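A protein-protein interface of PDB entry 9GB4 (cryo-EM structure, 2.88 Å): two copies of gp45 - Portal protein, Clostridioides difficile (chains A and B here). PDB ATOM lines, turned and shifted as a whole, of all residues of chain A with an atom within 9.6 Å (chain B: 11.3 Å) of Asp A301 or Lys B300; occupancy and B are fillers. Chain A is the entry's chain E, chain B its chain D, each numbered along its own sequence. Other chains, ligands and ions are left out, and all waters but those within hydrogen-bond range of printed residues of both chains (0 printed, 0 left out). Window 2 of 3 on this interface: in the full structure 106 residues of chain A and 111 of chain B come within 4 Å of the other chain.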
ATOM      1  N   LYS A 259     -27.728  21.923 -24.902  1.00  0.00           N
ATOM      2  CA  LYS A 259     -27.511  23.037 -23.989  1.00  0.00           C
ATOM      3  C   LYS A 259     -26.531  22.583 -22.922  1.00  0.00           C
ATOM      4  O   LYS A 259     -26.794  21.606 -22.215  1.00  0.00           O
ATOM      5  CB  LYS A 259     -28.850  23.493 -23.392  1.00  0.00           C
ATOM      6  CG  LYS A 259     -28.883  23.958 -21.928  1.00  0.00           C
ATOM      7  CD  LYS A 259     -30.323  24.157 -21.485  1.00  0.00           C
ATOM      8  CE  LYS A 259     -30.448  24.293 -19.983  1.00  0.00           C
ATOM      9  NZ  LYS A 259     -31.863  24.156 -19.556  1.00  0.00           N
ATOM     10  N   LEU A 260     -25.411  23.289 -22.809  1.00  0.00           N
ATOM     11  CA  LEU A 260     -24.386  23.008 -21.813  1.00  0.00           C
ATOM     12  C   LEU A 260     -24.293  24.195 -20.867  1.00  0.00           C
ATOM     13  O   LEU A 260     -24.030  25.320 -21.305  1.00  0.00           O
ATOM     14  CB  LEU A 260     -23.037  22.745 -22.479  1.00  0.00           C
ATOM     15  CG  LEU A 260     -22.992  21.609 -23.502  1.00  0.00           C
ATOM     16  CD1 LEU A 260     -21.607  21.492 -24.097  1.00  0.00           C
ATOM     17  CD2 LEU A 260     -23.402  20.295 -22.873  1.00  0.00           C
ATOM     18  N   LYS A 261     -24.508  23.942 -19.580  1.00  0.00           N
ATOM     19  CA  LYS A 261     -24.340  24.942 -18.533  1.00  0.00           C
ATOM     20  C   LYS A 261     -22.985  24.691 -17.886  1.00  0.00           C
ATOM     21  O   LYS A 261     -22.832  23.756 -17.095  1.00  0.00           O
ATOM     22  CB  LYS A 261     -25.477  24.861 -17.519  1.00  0.00           C
ATOM     23  CG  LYS A 261     -26.814  25.306 -18.087  1.00  0.00           C
ATOM     24  CD  LYS A 261     -27.979  24.909 -17.199  1.00  0.00           C
ATOM     25  CE  LYS A 261     -27.993  25.690 -15.899  1.00  0.00           C
ATOM     26  NZ  LYS A 261     -29.321  25.624 -15.232  1.00  0.00           N
ATOM     27  N   LEU A 262     -22.008  25.530 -18.223  1.00  0.00           N
ATOM     28  CA  LEU A 262     -20.604  25.273 -17.940  1.00  0.00           C
ATOM     29  C   LEU A 262     -20.077  26.248 -16.898  1.00  0.00           C
ATOM     30  O   LEU A 262     -20.684  27.287 -16.631  1.00  0.00           O
ATOM     31  CB  LEU A 262     -19.770  25.389 -19.216  1.00  0.00           C
ATOM     32  CG  LEU A 262     -20.143  24.419 -20.334  1.00  0.00           C
ATOM     33  CD1 LEU A 262     -19.482  24.840 -21.628  1.00  0.00           C
ATOM     34  CD2 LEU A 262     -19.755  22.999 -19.966  1.00  0.00           C
ATOM     35  N   THR A 263     -18.944  25.892 -16.292  1.00  0.00           N
ATOM     36  CA  THR A 263     -18.282  26.811 -15.373  1.00  0.00           C
ATOM     37  C   THR A 263     -17.542  27.905 -16.132  1.00  0.00           C
ATOM     38  O   THR A 263     -17.494  29.055 -15.681  1.00  0.00           O
ATOM     39  CB  THR A 263     -17.322  26.046 -14.463  1.00  0.00           C
ATOM     40  OG1 THR A 263     -18.034  25.009 -13.780  1.00  0.00           O
ATOM     41  CG2 THR A 263     -16.698  26.978 -13.438  1.00  0.00           C
ATOM     42  N   ASP A 264     -16.956  27.566 -17.282  1.00  0.00           N
ATOM     43  CA  ASP A 264     -16.226  28.533 -18.100  1.00  0.00           C
ATOM     44  C   ASP A 264     -16.464  28.151 -19.559  1.00  0.00           C
ATOM     45  O   ASP A 264     -15.890  27.174 -20.047  1.00  0.00           O
ATOM     46  CB  ASP A 264     -14.744  28.537 -17.752  1.00  0.00           C
ATOM     47  CG  ASP A 264     -14.007  29.727 -18.337  1.00  0.00           C
ATOM     48  OD1 ASP A 264     -14.564  30.402 -19.227  1.00  0.00           O
ATOM     49  OD2 ASP A 264     -12.865  29.989 -17.904  1.00  0.00           O
ATOM     50  N   VAL A 265     -17.310  28.923 -20.242  1.00  0.00           N
ATOM     51  CA  VAL A 265     -17.710  28.572 -21.603  1.00  0.00           C
ATOM     52  C   VAL A 265     -16.533  28.710 -22.560  1.00  0.00           C
ATOM     53  O   VAL A 265     -16.258  27.814 -23.368  1.00  0.00           O
ATOM     54  CB  VAL A 265     -18.902  29.437 -22.050  1.00  0.00           C
ATOM     55  CG1 VAL A 265     -19.174  29.250 -23.534  1.00  0.00           C
ATOM     56  CG2 VAL A 265     -20.149  29.101 -21.242  1.00  0.00           C
ATOM     57  N   LEU A 298     -17.930  16.174 -17.153  1.00  0.00           N
ATOM     58  CA  LEU A 298     -18.291  17.473 -16.607  1.00  0.00           C
ATOM     59  C   LEU A 298     -17.977  17.507 -15.119  1.00  0.00           C
ATOM     60  O   LEU A 298     -17.800  16.472 -14.476  1.00  0.00           O
ATOM     61  CB  LEU A 298     -19.778  17.772 -16.835  1.00  0.00           C
ATOM     62  CG  LEU A 298     -20.277  17.790 -18.281  1.00  0.00           C
ATOM     63  CD1 LEU A 298     -21.785  17.921 -18.306  1.00  0.00           C
ATOM     64  CD2 LEU A 298     -19.638  18.911 -19.076  1.00  0.00           C
ATOM     65  N   ASN A 299     -17.896  18.720 -14.583  1.00  0.00           N
ATOM     66  CA  ASN A 299     -17.729  18.898 -13.150  1.00  0.00           C
ATOM     67  C   ASN A 299     -19.057  18.652 -12.437  1.00  0.00           C
ATOM     68  O   ASN A 299     -20.086  18.383 -13.055  1.00  0.00           O
ATOM     69  CB  ASN A 299     -17.219  20.303 -12.839  1.00  0.00           C
ATOM     70  CG  ASN A 299     -16.021  20.697 -13.685  1.00  0.00           C
ATOM     71  OD1 ASN A 299     -15.923  21.839 -14.133  1.00  0.00           O
ATOM     72  ND2 ASN A 299     -15.095  19.765 -13.891  1.00  0.00           N
ATOM     73  N   LYS A 300     -19.020  18.742 -11.106  1.00  0.00           N
ATOM     74  CA  LYS A 300     -20.243  18.580 -10.327  1.00  0.00           C
ATOM     75  C   LYS A 300     -21.253  19.670 -10.654  1.00  0.00           C
ATOM     76  O   LYS A 300     -22.449  19.399 -10.797  1.00  0.00           O
ATOM     77  CB  LYS A 300     -19.928  18.601  -8.833  1.00  0.00           C
ATOM     78  CG  LYS A 300     -18.941  17.557  -8.361  1.00  0.00           C
ATOM     79  CD  LYS A 300     -18.797  17.636  -6.851  1.00  0.00           C
ATOM     80  CE  LYS A 300     -17.546  16.944  -6.355  1.00  0.00           C
ATOM     81  NZ  LYS A 300     -17.339  17.176  -4.899  1.00  0.00           N
ATOM     82  N   ASP A 301     -20.788  20.913 -10.769  1.00  0.00           N
ATOM     83  CA  ASP A 301     -21.687  22.041 -10.967  1.00  0.00           C
ATOM     84  C   ASP A 301     -22.218  22.132 -12.388  1.00  0.00           C
ATOM     85  O   ASP A 301     -23.336  22.619 -12.587  1.00  0.00           O
ATOM     86  CB  ASP A 301     -20.967  23.344 -10.614  1.00  0.00           C
ATOM     87  CG  ASP A 301     -20.313  23.296  -9.250  1.00  0.00           C
ATOM     88  OD1 ASP A 301     -20.766  22.498  -8.402  1.00  0.00           O
ATOM     89  OD2 ASP A 301     -19.344  24.051  -9.027  1.00  0.00           O
ATOM     90  N   GLU A 302     -21.453  21.676 -13.372  1.00  0.00           N
ATOM     91  CA  GLU A 302     -21.839  21.817 -14.765  1.00  0.00           C
ATOM     92  C   GLU A 302     -22.976  20.862 -15.104  1.00  0.00           C
ATOM     93  O   GLU A 302     -23.084  19.768 -14.544  1.00  0.00           O
ATOM     94  CB  GLU A 302     -20.637  21.554 -15.669  1.00  0.00           C
ATOM     95  CG  GLU A 302     -19.490  22.525 -15.453  1.00  0.00           C
ATOM     96  CD  GLU A 302     -18.308  22.255 -16.362  1.00  0.00           C
ATOM     97  OE1 GLU A 302     -17.944  21.075 -16.535  1.00  0.00           O
ATOM     98  OE2 GLU A 302     -17.737  23.226 -16.901  1.00  0.00           O
ATOM     99  N   GLU A 303     -23.832  21.292 -16.031  1.00  0.00           N
ATOM    100  CA  GLU A 303     -25.026  20.553 -16.412  1.00  0.00           C
ATOM    101  C   GLU A 303     -25.156  20.574 -17.927  1.00  0.00           C
ATOM    102  O   GLU A 303     -24.770  21.545 -18.581  1.00  0.00           O
ATOM    103  CB  GLU A 303     -26.277  21.162 -15.754  1.00  0.00           C
ATOM    104  CG  GLU A 303     -27.592  20.426 -16.005  1.00  0.00           C
ATOM    105  CD  GLU A 303     -27.665  19.087 -15.301  1.00  0.00           C
ATOM    106  OE1 GLU A 303     -26.700  18.723 -14.598  1.00  0.00           O
ATOM    107  OE2 GLU A 303     -28.693  18.394 -15.448  1.00  0.00           O
ATOM    108  N   ALA A 304     -25.696  19.487 -18.477  1.00  0.00           N
ATOM    109  CA  ALA A 304     -25.946  19.365 -19.907  1.00  0.00           C
ATOM    110  C   ALA A 304     -27.346  18.814 -20.118  1.00  0.00           C
ATOM    111  O   ALA A 304     -27.767  17.886 -19.424  1.00  0.00           O
ATOM    112  CB  ALA A 304     -24.919  18.456 -20.587  1.00  0.00           C
ATOM    113  N   LYS B 261     -32.667  32.794 -20.779  1.00  0.00           N
ATOM    114  CA  LYS B 261     -32.534  33.576 -19.556  1.00  0.00           C
ATOM    115  C   LYS B 261     -31.044  33.754 -19.307  1.00  0.00           C
ATOM    116  O   LYS B 261     -30.358  32.803 -18.917  1.00  0.00           O
ATOM    117  CB  LYS B 261     -33.228  32.883 -18.387  1.00  0.00           C
ATOM    118  CG  LYS B 261     -34.739  32.838 -18.532  1.00  0.00           C
ATOM    119  CD  LYS B 261     -35.380  31.840 -17.587  1.00  0.00           C
ATOM    120  CE  LYS B 261     -35.262  32.279 -16.142  1.00  0.00           C
ATOM    121  NZ  LYS B 261     -36.196  31.531 -15.259  1.00  0.00           N
ATOM    122  N   LEU B 262     -30.550  34.970 -19.526  1.00  0.00           N
ATOM    123  CA  LEU B 262     -29.126  35.243 -19.634  1.00  0.00           C
ATOM    124  C   LEU B 262     -28.680  36.195 -18.536  1.00  0.00           C
ATOM    125  O   LEU B 262     -29.476  36.970 -18.000  1.00  0.00           O
ATOM    126  CB  LEU B 262     -28.790  35.851 -20.997  1.00  0.00           C
ATOM    127  CG  LEU B 262     -29.197  35.029 -22.216  1.00  0.00           C
ATOM    128  CD1 LEU B 262     -29.039  35.858 -23.471  1.00  0.00           C
ATOM    129  CD2 LEU B 262     -28.377  33.756 -22.303  1.00  0.00           C
ATOM    130  N   THR B 263     -27.390  36.124 -18.206  1.00  0.00           N
ATOM    131  CA  THR B 263     -26.816  37.075 -17.261  1.00  0.00           C
ATOM    132  C   THR B 263     -26.755  38.475 -17.858  1.00  0.00           C
ATOM    133  O   THR B 263     -26.958  39.466 -17.147  1.00  0.00           O
ATOM    134  CB  THR B 263     -25.420  36.619 -16.838  1.00  0.00           C
ATOM    135  OG1 THR B 263     -25.437  35.218 -16.542  1.00  0.00           O
ATOM    136  CG2 THR B 263     -24.943  37.392 -15.620  1.00  0.00           C
ATOM    137  N   ASP B 264     -26.473  38.576 -19.156  1.00  0.00           N
ATOM    138  CA  ASP B 264     -26.325  39.869 -19.820  1.00  0.00           C
ATOM    139  C   ASP B 264     -26.816  39.707 -21.251  1.00  0.00           C
ATOM    140  O   ASP B 264     -26.109  39.141 -22.089  1.00  0.00           O
ATOM    141  CB  ASP B 264     -24.873  40.336 -19.770  1.00  0.00           C
ATOM    142  CG  ASP B 264     -24.693  41.763 -20.260  1.00  0.00           C
ATOM    143  OD1 ASP B 264     -25.063  42.061 -21.414  1.00  0.00           O
ATOM    144  OD2 ASP B 264     -24.173  42.592 -19.484  1.00  0.00           O
ATOM    145  N   LEU B 296     -25.970  25.333 -27.653  1.00  0.00           N
ATOM    146  CA  LEU B 296     -25.989  26.409 -26.670  1.00  0.00           C
ATOM    147  C   LEU B 296     -24.937  26.138 -25.607  1.00  0.00           C
ATOM    148  O   LEU B 296     -25.024  25.140 -24.885  1.00  0.00           O
ATOM    149  CB  LEU B 296     -27.369  26.536 -26.024  1.00  0.00           C
ATOM    150  CG  LEU B 296     -28.462  27.256 -26.816  1.00  0.00           C
ATOM    151  CD1 LEU B 296     -28.821  26.501 -28.076  1.00  0.00           C
ATOM    152  CD2 LEU B 296     -29.690  27.450 -25.948  1.00  0.00           C
ATOM    153  N   PHE B 297     -23.950  27.025 -25.515  1.00  0.00           N
ATOM    154  CA  PHE B 297     -22.980  27.036 -24.429  1.00  0.00           C
ATOM    155  C   PHE B 297     -23.339  28.180 -23.497  1.00  0.00           C
ATOM    156  O   PHE B 297     -23.374  29.340 -23.920  1.00  0.00           O
ATOM    157  CB  PHE B 297     -21.556  27.203 -24.953  1.00  0.00           C
ATOM    158  CG  PHE B 297     -21.151  26.167 -25.954  1.00  0.00           C
ATOM    159  CD1 PHE B 297     -20.611  24.966 -25.543  1.00  0.00           C
ATOM    160  CD2 PHE B 297     -21.299  26.399 -27.306  1.00  0.00           C
ATOM    161  CE1 PHE B 297     -20.232  24.015 -26.460  1.00  0.00           C
ATOM    162  CE2 PHE B 297     -20.922  25.448 -28.227  1.00  0.00           C
ATOM    163  CZ  PHE B 297     -20.388  24.255 -27.802  1.00  0.00           C
ATOM    164  N   LEU B 298     -23.595  27.854 -22.234  1.00  0.00           N
ATOM    165  CA  LEU B 298     -24.094  28.805 -21.254  1.00  0.00           C
ATOM    166  C   LEU B 298     -23.307  28.648 -19.965  1.00  0.00           C
ATOM    167  O   LEU B 298     -22.775  27.570 -19.689  1.00  0.00           O
ATOM    168  CB  LEU B 298     -25.584  28.577 -20.983  1.00  0.00           C
ATOM    169  CG  LEU B 298     -26.533  28.627 -22.182  1.00  0.00           C
ATOM    170  CD1 LEU B 298     -27.930  28.236 -21.749  1.00  0.00           C
ATOM    171  CD2 LEU B 298     -26.549  29.999 -22.826  1.00  0.00           C
ATOM    172  N   ASN B 299     -23.217  29.722 -19.188  1.00  0.00           N
ATOM    173  CA  ASN B 299     -22.679  29.592 -17.844  1.00  0.00           C
ATOM    174  C   ASN B 299     -23.751  29.022 -16.919  1.00  0.00           C
ATOM    175  O   ASN B 299     -24.907  28.842 -17.307  1.00  0.00           O
ATOM    176  CB  ASN B 299     -22.153  30.930 -17.318  1.00  0.00           C
ATOM    177  CG  ASN B 299     -23.192  32.022 -17.336  1.00  0.00           C
ATOM    178  OD1 ASN B 299     -23.447  32.629 -18.374  1.00  0.00           O
ATOM    179  ND2 ASN B 299     -23.796  32.285 -16.185  1.00  0.00           N
ATOM    180  N   LYS B 300     -23.351  28.726 -15.681  1.00  0.00           N
ATOM    181  CA  LYS B 300     -24.204  27.944 -14.790  1.00  0.00           C
ATOM    182  C   LYS B 300     -25.508  28.657 -14.460  1.00  0.00           C
ATOM    183  O   LYS B 300     -26.543  28.005 -14.286  1.00  0.00           O
ATOM    184  CB  LYS B 300     -23.456  27.619 -13.498  1.00  0.00           C
ATOM    185  CG  LYS B 300     -22.147  26.873 -13.705  1.00  0.00           C
ATOM    186  CD  LYS B 300     -21.532  26.419 -12.385  1.00  0.00           C
ATOM    187  CE  LYS B 300     -21.032  27.586 -11.542  1.00  0.00           C
ATOM    188  NZ  LYS B 300     -20.415  27.125 -10.268  1.00  0.00           N
ATOM    189  N   ASP B 301     -25.484  29.986 -14.365  1.00  0.00           N
ATOM    190  CA  ASP B 301     -26.678  30.713 -13.945  1.00  0.00           C
ATOM    191  C   ASP B 301     -27.731  30.770 -15.045  1.00  0.00           C
ATOM    192  O   ASP B 301     -28.931  30.751 -14.751  1.00  0.00           O
ATOM    193  CB  ASP B 301     -26.298  32.126 -13.511  1.00  0.00           C
ATOM    194  CG  ASP B 301     -25.405  32.138 -12.289  1.00  0.00           C
ATOM    195  OD1 ASP B 301     -25.086  31.045 -11.775  1.00  0.00           O
ATOM    196  OD2 ASP B 301     -25.019  33.238 -11.842  1.00  0.00           O
ATOM    197  N   GLU B 302     -27.310  30.839 -16.302  1.00  0.00           N
ATOM    198  CA  GLU B 302     -28.234  31.037 -17.406  1.00  0.00           C
ATOM    199  C   GLU B 302     -29.038  29.773 -17.683  1.00  0.00           C
ATOM    200  O   GLU B 302     -28.621  28.658 -17.355  1.00  0.00           O
ATOM    201  CB  GLU B 302     -27.472  31.458 -18.660  1.00  0.00           C
ATOM    202  CG  GLU B 302     -26.619  32.693 -18.451  1.00  0.00           C
ATOM    203  CD  GLU B 302     -26.005  33.213 -19.734  1.00  0.00           C
ATOM    204  OE1 GLU B 302     -25.769  32.405 -20.655  1.00  0.00           O
ATOM    205  OE2 GLU B 302     -25.748  34.431 -19.819  1.00  0.00           O
ATOM    206  N   GLU B 303     -30.206  29.961 -18.294  1.00  0.00           N
ATOM    207  CA  GLU B 303     -31.133  28.880 -18.590  1.00  0.00           C
ATOM    208  C   GLU B 303     -31.741  29.125 -19.962  1.00  0.00           C
ATOM    209  O   GLU B 303     -31.912  30.270 -20.382  1.00  0.00           O
ATOM    210  CB  GLU B 303     -32.231  28.790 -17.517  1.00  0.00           C
ATOM    211  CG  GLU B 303     -33.225  27.640 -17.663  1.00  0.00           C
ATOM    212  CD  GLU B 303     -32.612  26.283 -17.378  1.00  0.00           C
ATOM    213  OE1 GLU B 303     -31.396  26.218 -17.104  1.00  0.00           O
ATOM    214  OE2 GLU B 303     -33.349  25.277 -17.428  1.00  0.00           O
ATOM    215  N   ALA B 304     -32.057  28.034 -20.659  1.00  0.00           N
ATOM    216  CA  ALA B 304     -32.692  28.091 -21.969  1.00  0.00           C
ATOM    217  C   ALA B 304     -33.837  27.093 -22.012  1.00  0.00           C
ATOM    218  O   ALA B 304     -33.722  25.982 -21.491  1.00  0.00           O
ATOM    219  CB  ALA B 304     -31.697  27.792 -23.094  1.00  0.00           C
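Among the printed residues, merely in contact across the chains: Lys A261 with Lys B300, Lys A261 with Leu B298, Leu A262 with Asn B299, Lys A261 with Glu B302, Lys A259 with Leu B296, Val A265 with Leu B298, Val A265 with Phe B297, Leu A260 with Phe B297 and Val A265 with Asn B299.
N of Lys B261 sits at hydrogen-bond distance from O of Glu B303. The side-chain amide nitrogen (ND2) of Asn B299 sits at hydrogen-bond distance from the side-chain hydroxyl (OG1) of Thr B263 (3.4 Å). OE2 of Glu B302 lies within hydrogen-bond range of N of Thr B263, 2.9 Å away. The side-chain amide nitrogen of Asn B299 sits close to the backbone NH of Asp B301 (3.4 Å). OE2 of Glu B302 lies close to OD1 of Asn B299, 3.3 Å away. O of Glu A303 is in hydrogen-bond range of N of Lys A261 (2.6 Å).
The backbone NH of Leu A260 is in hydrogen-bond range of the backbone carbonyl oxygen of Leu B296. The backbone NH (N) of Leu B298 lies within hydrogen-bond range of the backbone carbonyl oxygen (O) of Leu A260 (2.7 Å). O of Leu B298 is in hydrogen-bond range of N of Leu A262 (2.6 Å). N of Lys B300 sits at hydrogen-bond distance from O of Leu A262. OD2 of Asp A301 is in salt-bridge range of NZ of Lys B300 (3.5 Å). NZ of Lys A259 lies within salt-bridge range of OE2 of Glu B303. OE1 of Glu B303 lies within salt-bridge range of NZ of Lys A261. The backbone carbonyl oxygen of Ala B304 is in hydrogen-bond range of the side-chain amino group of Lys A259.
Hydrophobic or aromatic side chains of chain B within 4 Å of the printed part of chain A: Phe B297 and Leu B298. Among the printed residues, Asp or Glu carboxylates within 4 Å of a Lys or Arg side-chain nitrogen of the other chain: Lys A259 with Glu B303, Lys A261 with Glu B303 and Asp A301 with Lys B300.
Lys A261 touches Glu B303, but with the chains exchanged Glu A303 does not touch Lys B261 (12.6 Å). Leu A262 touches Asn B299, but with the chains exchanged Asn A299 does not touch Leu B262 (19.1 Å). Leu A262 touches Lys B300, but with the chains exchanged Lys A300 does not touch Leu B262 (19.3 Å). Asp A301 touches Lys B300, but with the chains exchanged Lys A300 does not touch Asp B301 (11.6 Å). Positions printed for both chains: 261, 262, 263, 264, 298, 299, 300, 301, 302, 303 and 304. Of the 17 pairs that touch across the chains among the printed residues, none has its exchanged pair printed and touching as well.
Of the printed residues of chain B, Leu A262 touches Leu B298 (2.6 Å), Asn B299 (3.3 Å) and Lys B300 (3.2 Å). Printed residues of chain B within 4 Å of Val A265: Phe B297, Leu B298 and Asn B299. No residue of chain B comes within 4 Å of Asn A299. No residue of chain B comes within 4 Å of Lys A300. Asp A301 touches just one residue of chain B: Lys B300. No residue of chain B comes within 4 Å of Glu A302. Printed residues of chain A within 4 Å of Leu B298: Leu A260 (2.7 Å), Lys A261 (3.3 Å), Leu A262 (2.6 Å) and Val A265 (3.4 Å). Of chain A, only Lys A261, Leu A262 and Asp A301 come within 4 Å of Lys B300. Printed residues of chain A within 4 Å of Ala B304: Lys A259. The nearest printed residue of chain B that does not touch Lys A259 is Leu B298 (4.4 Å).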
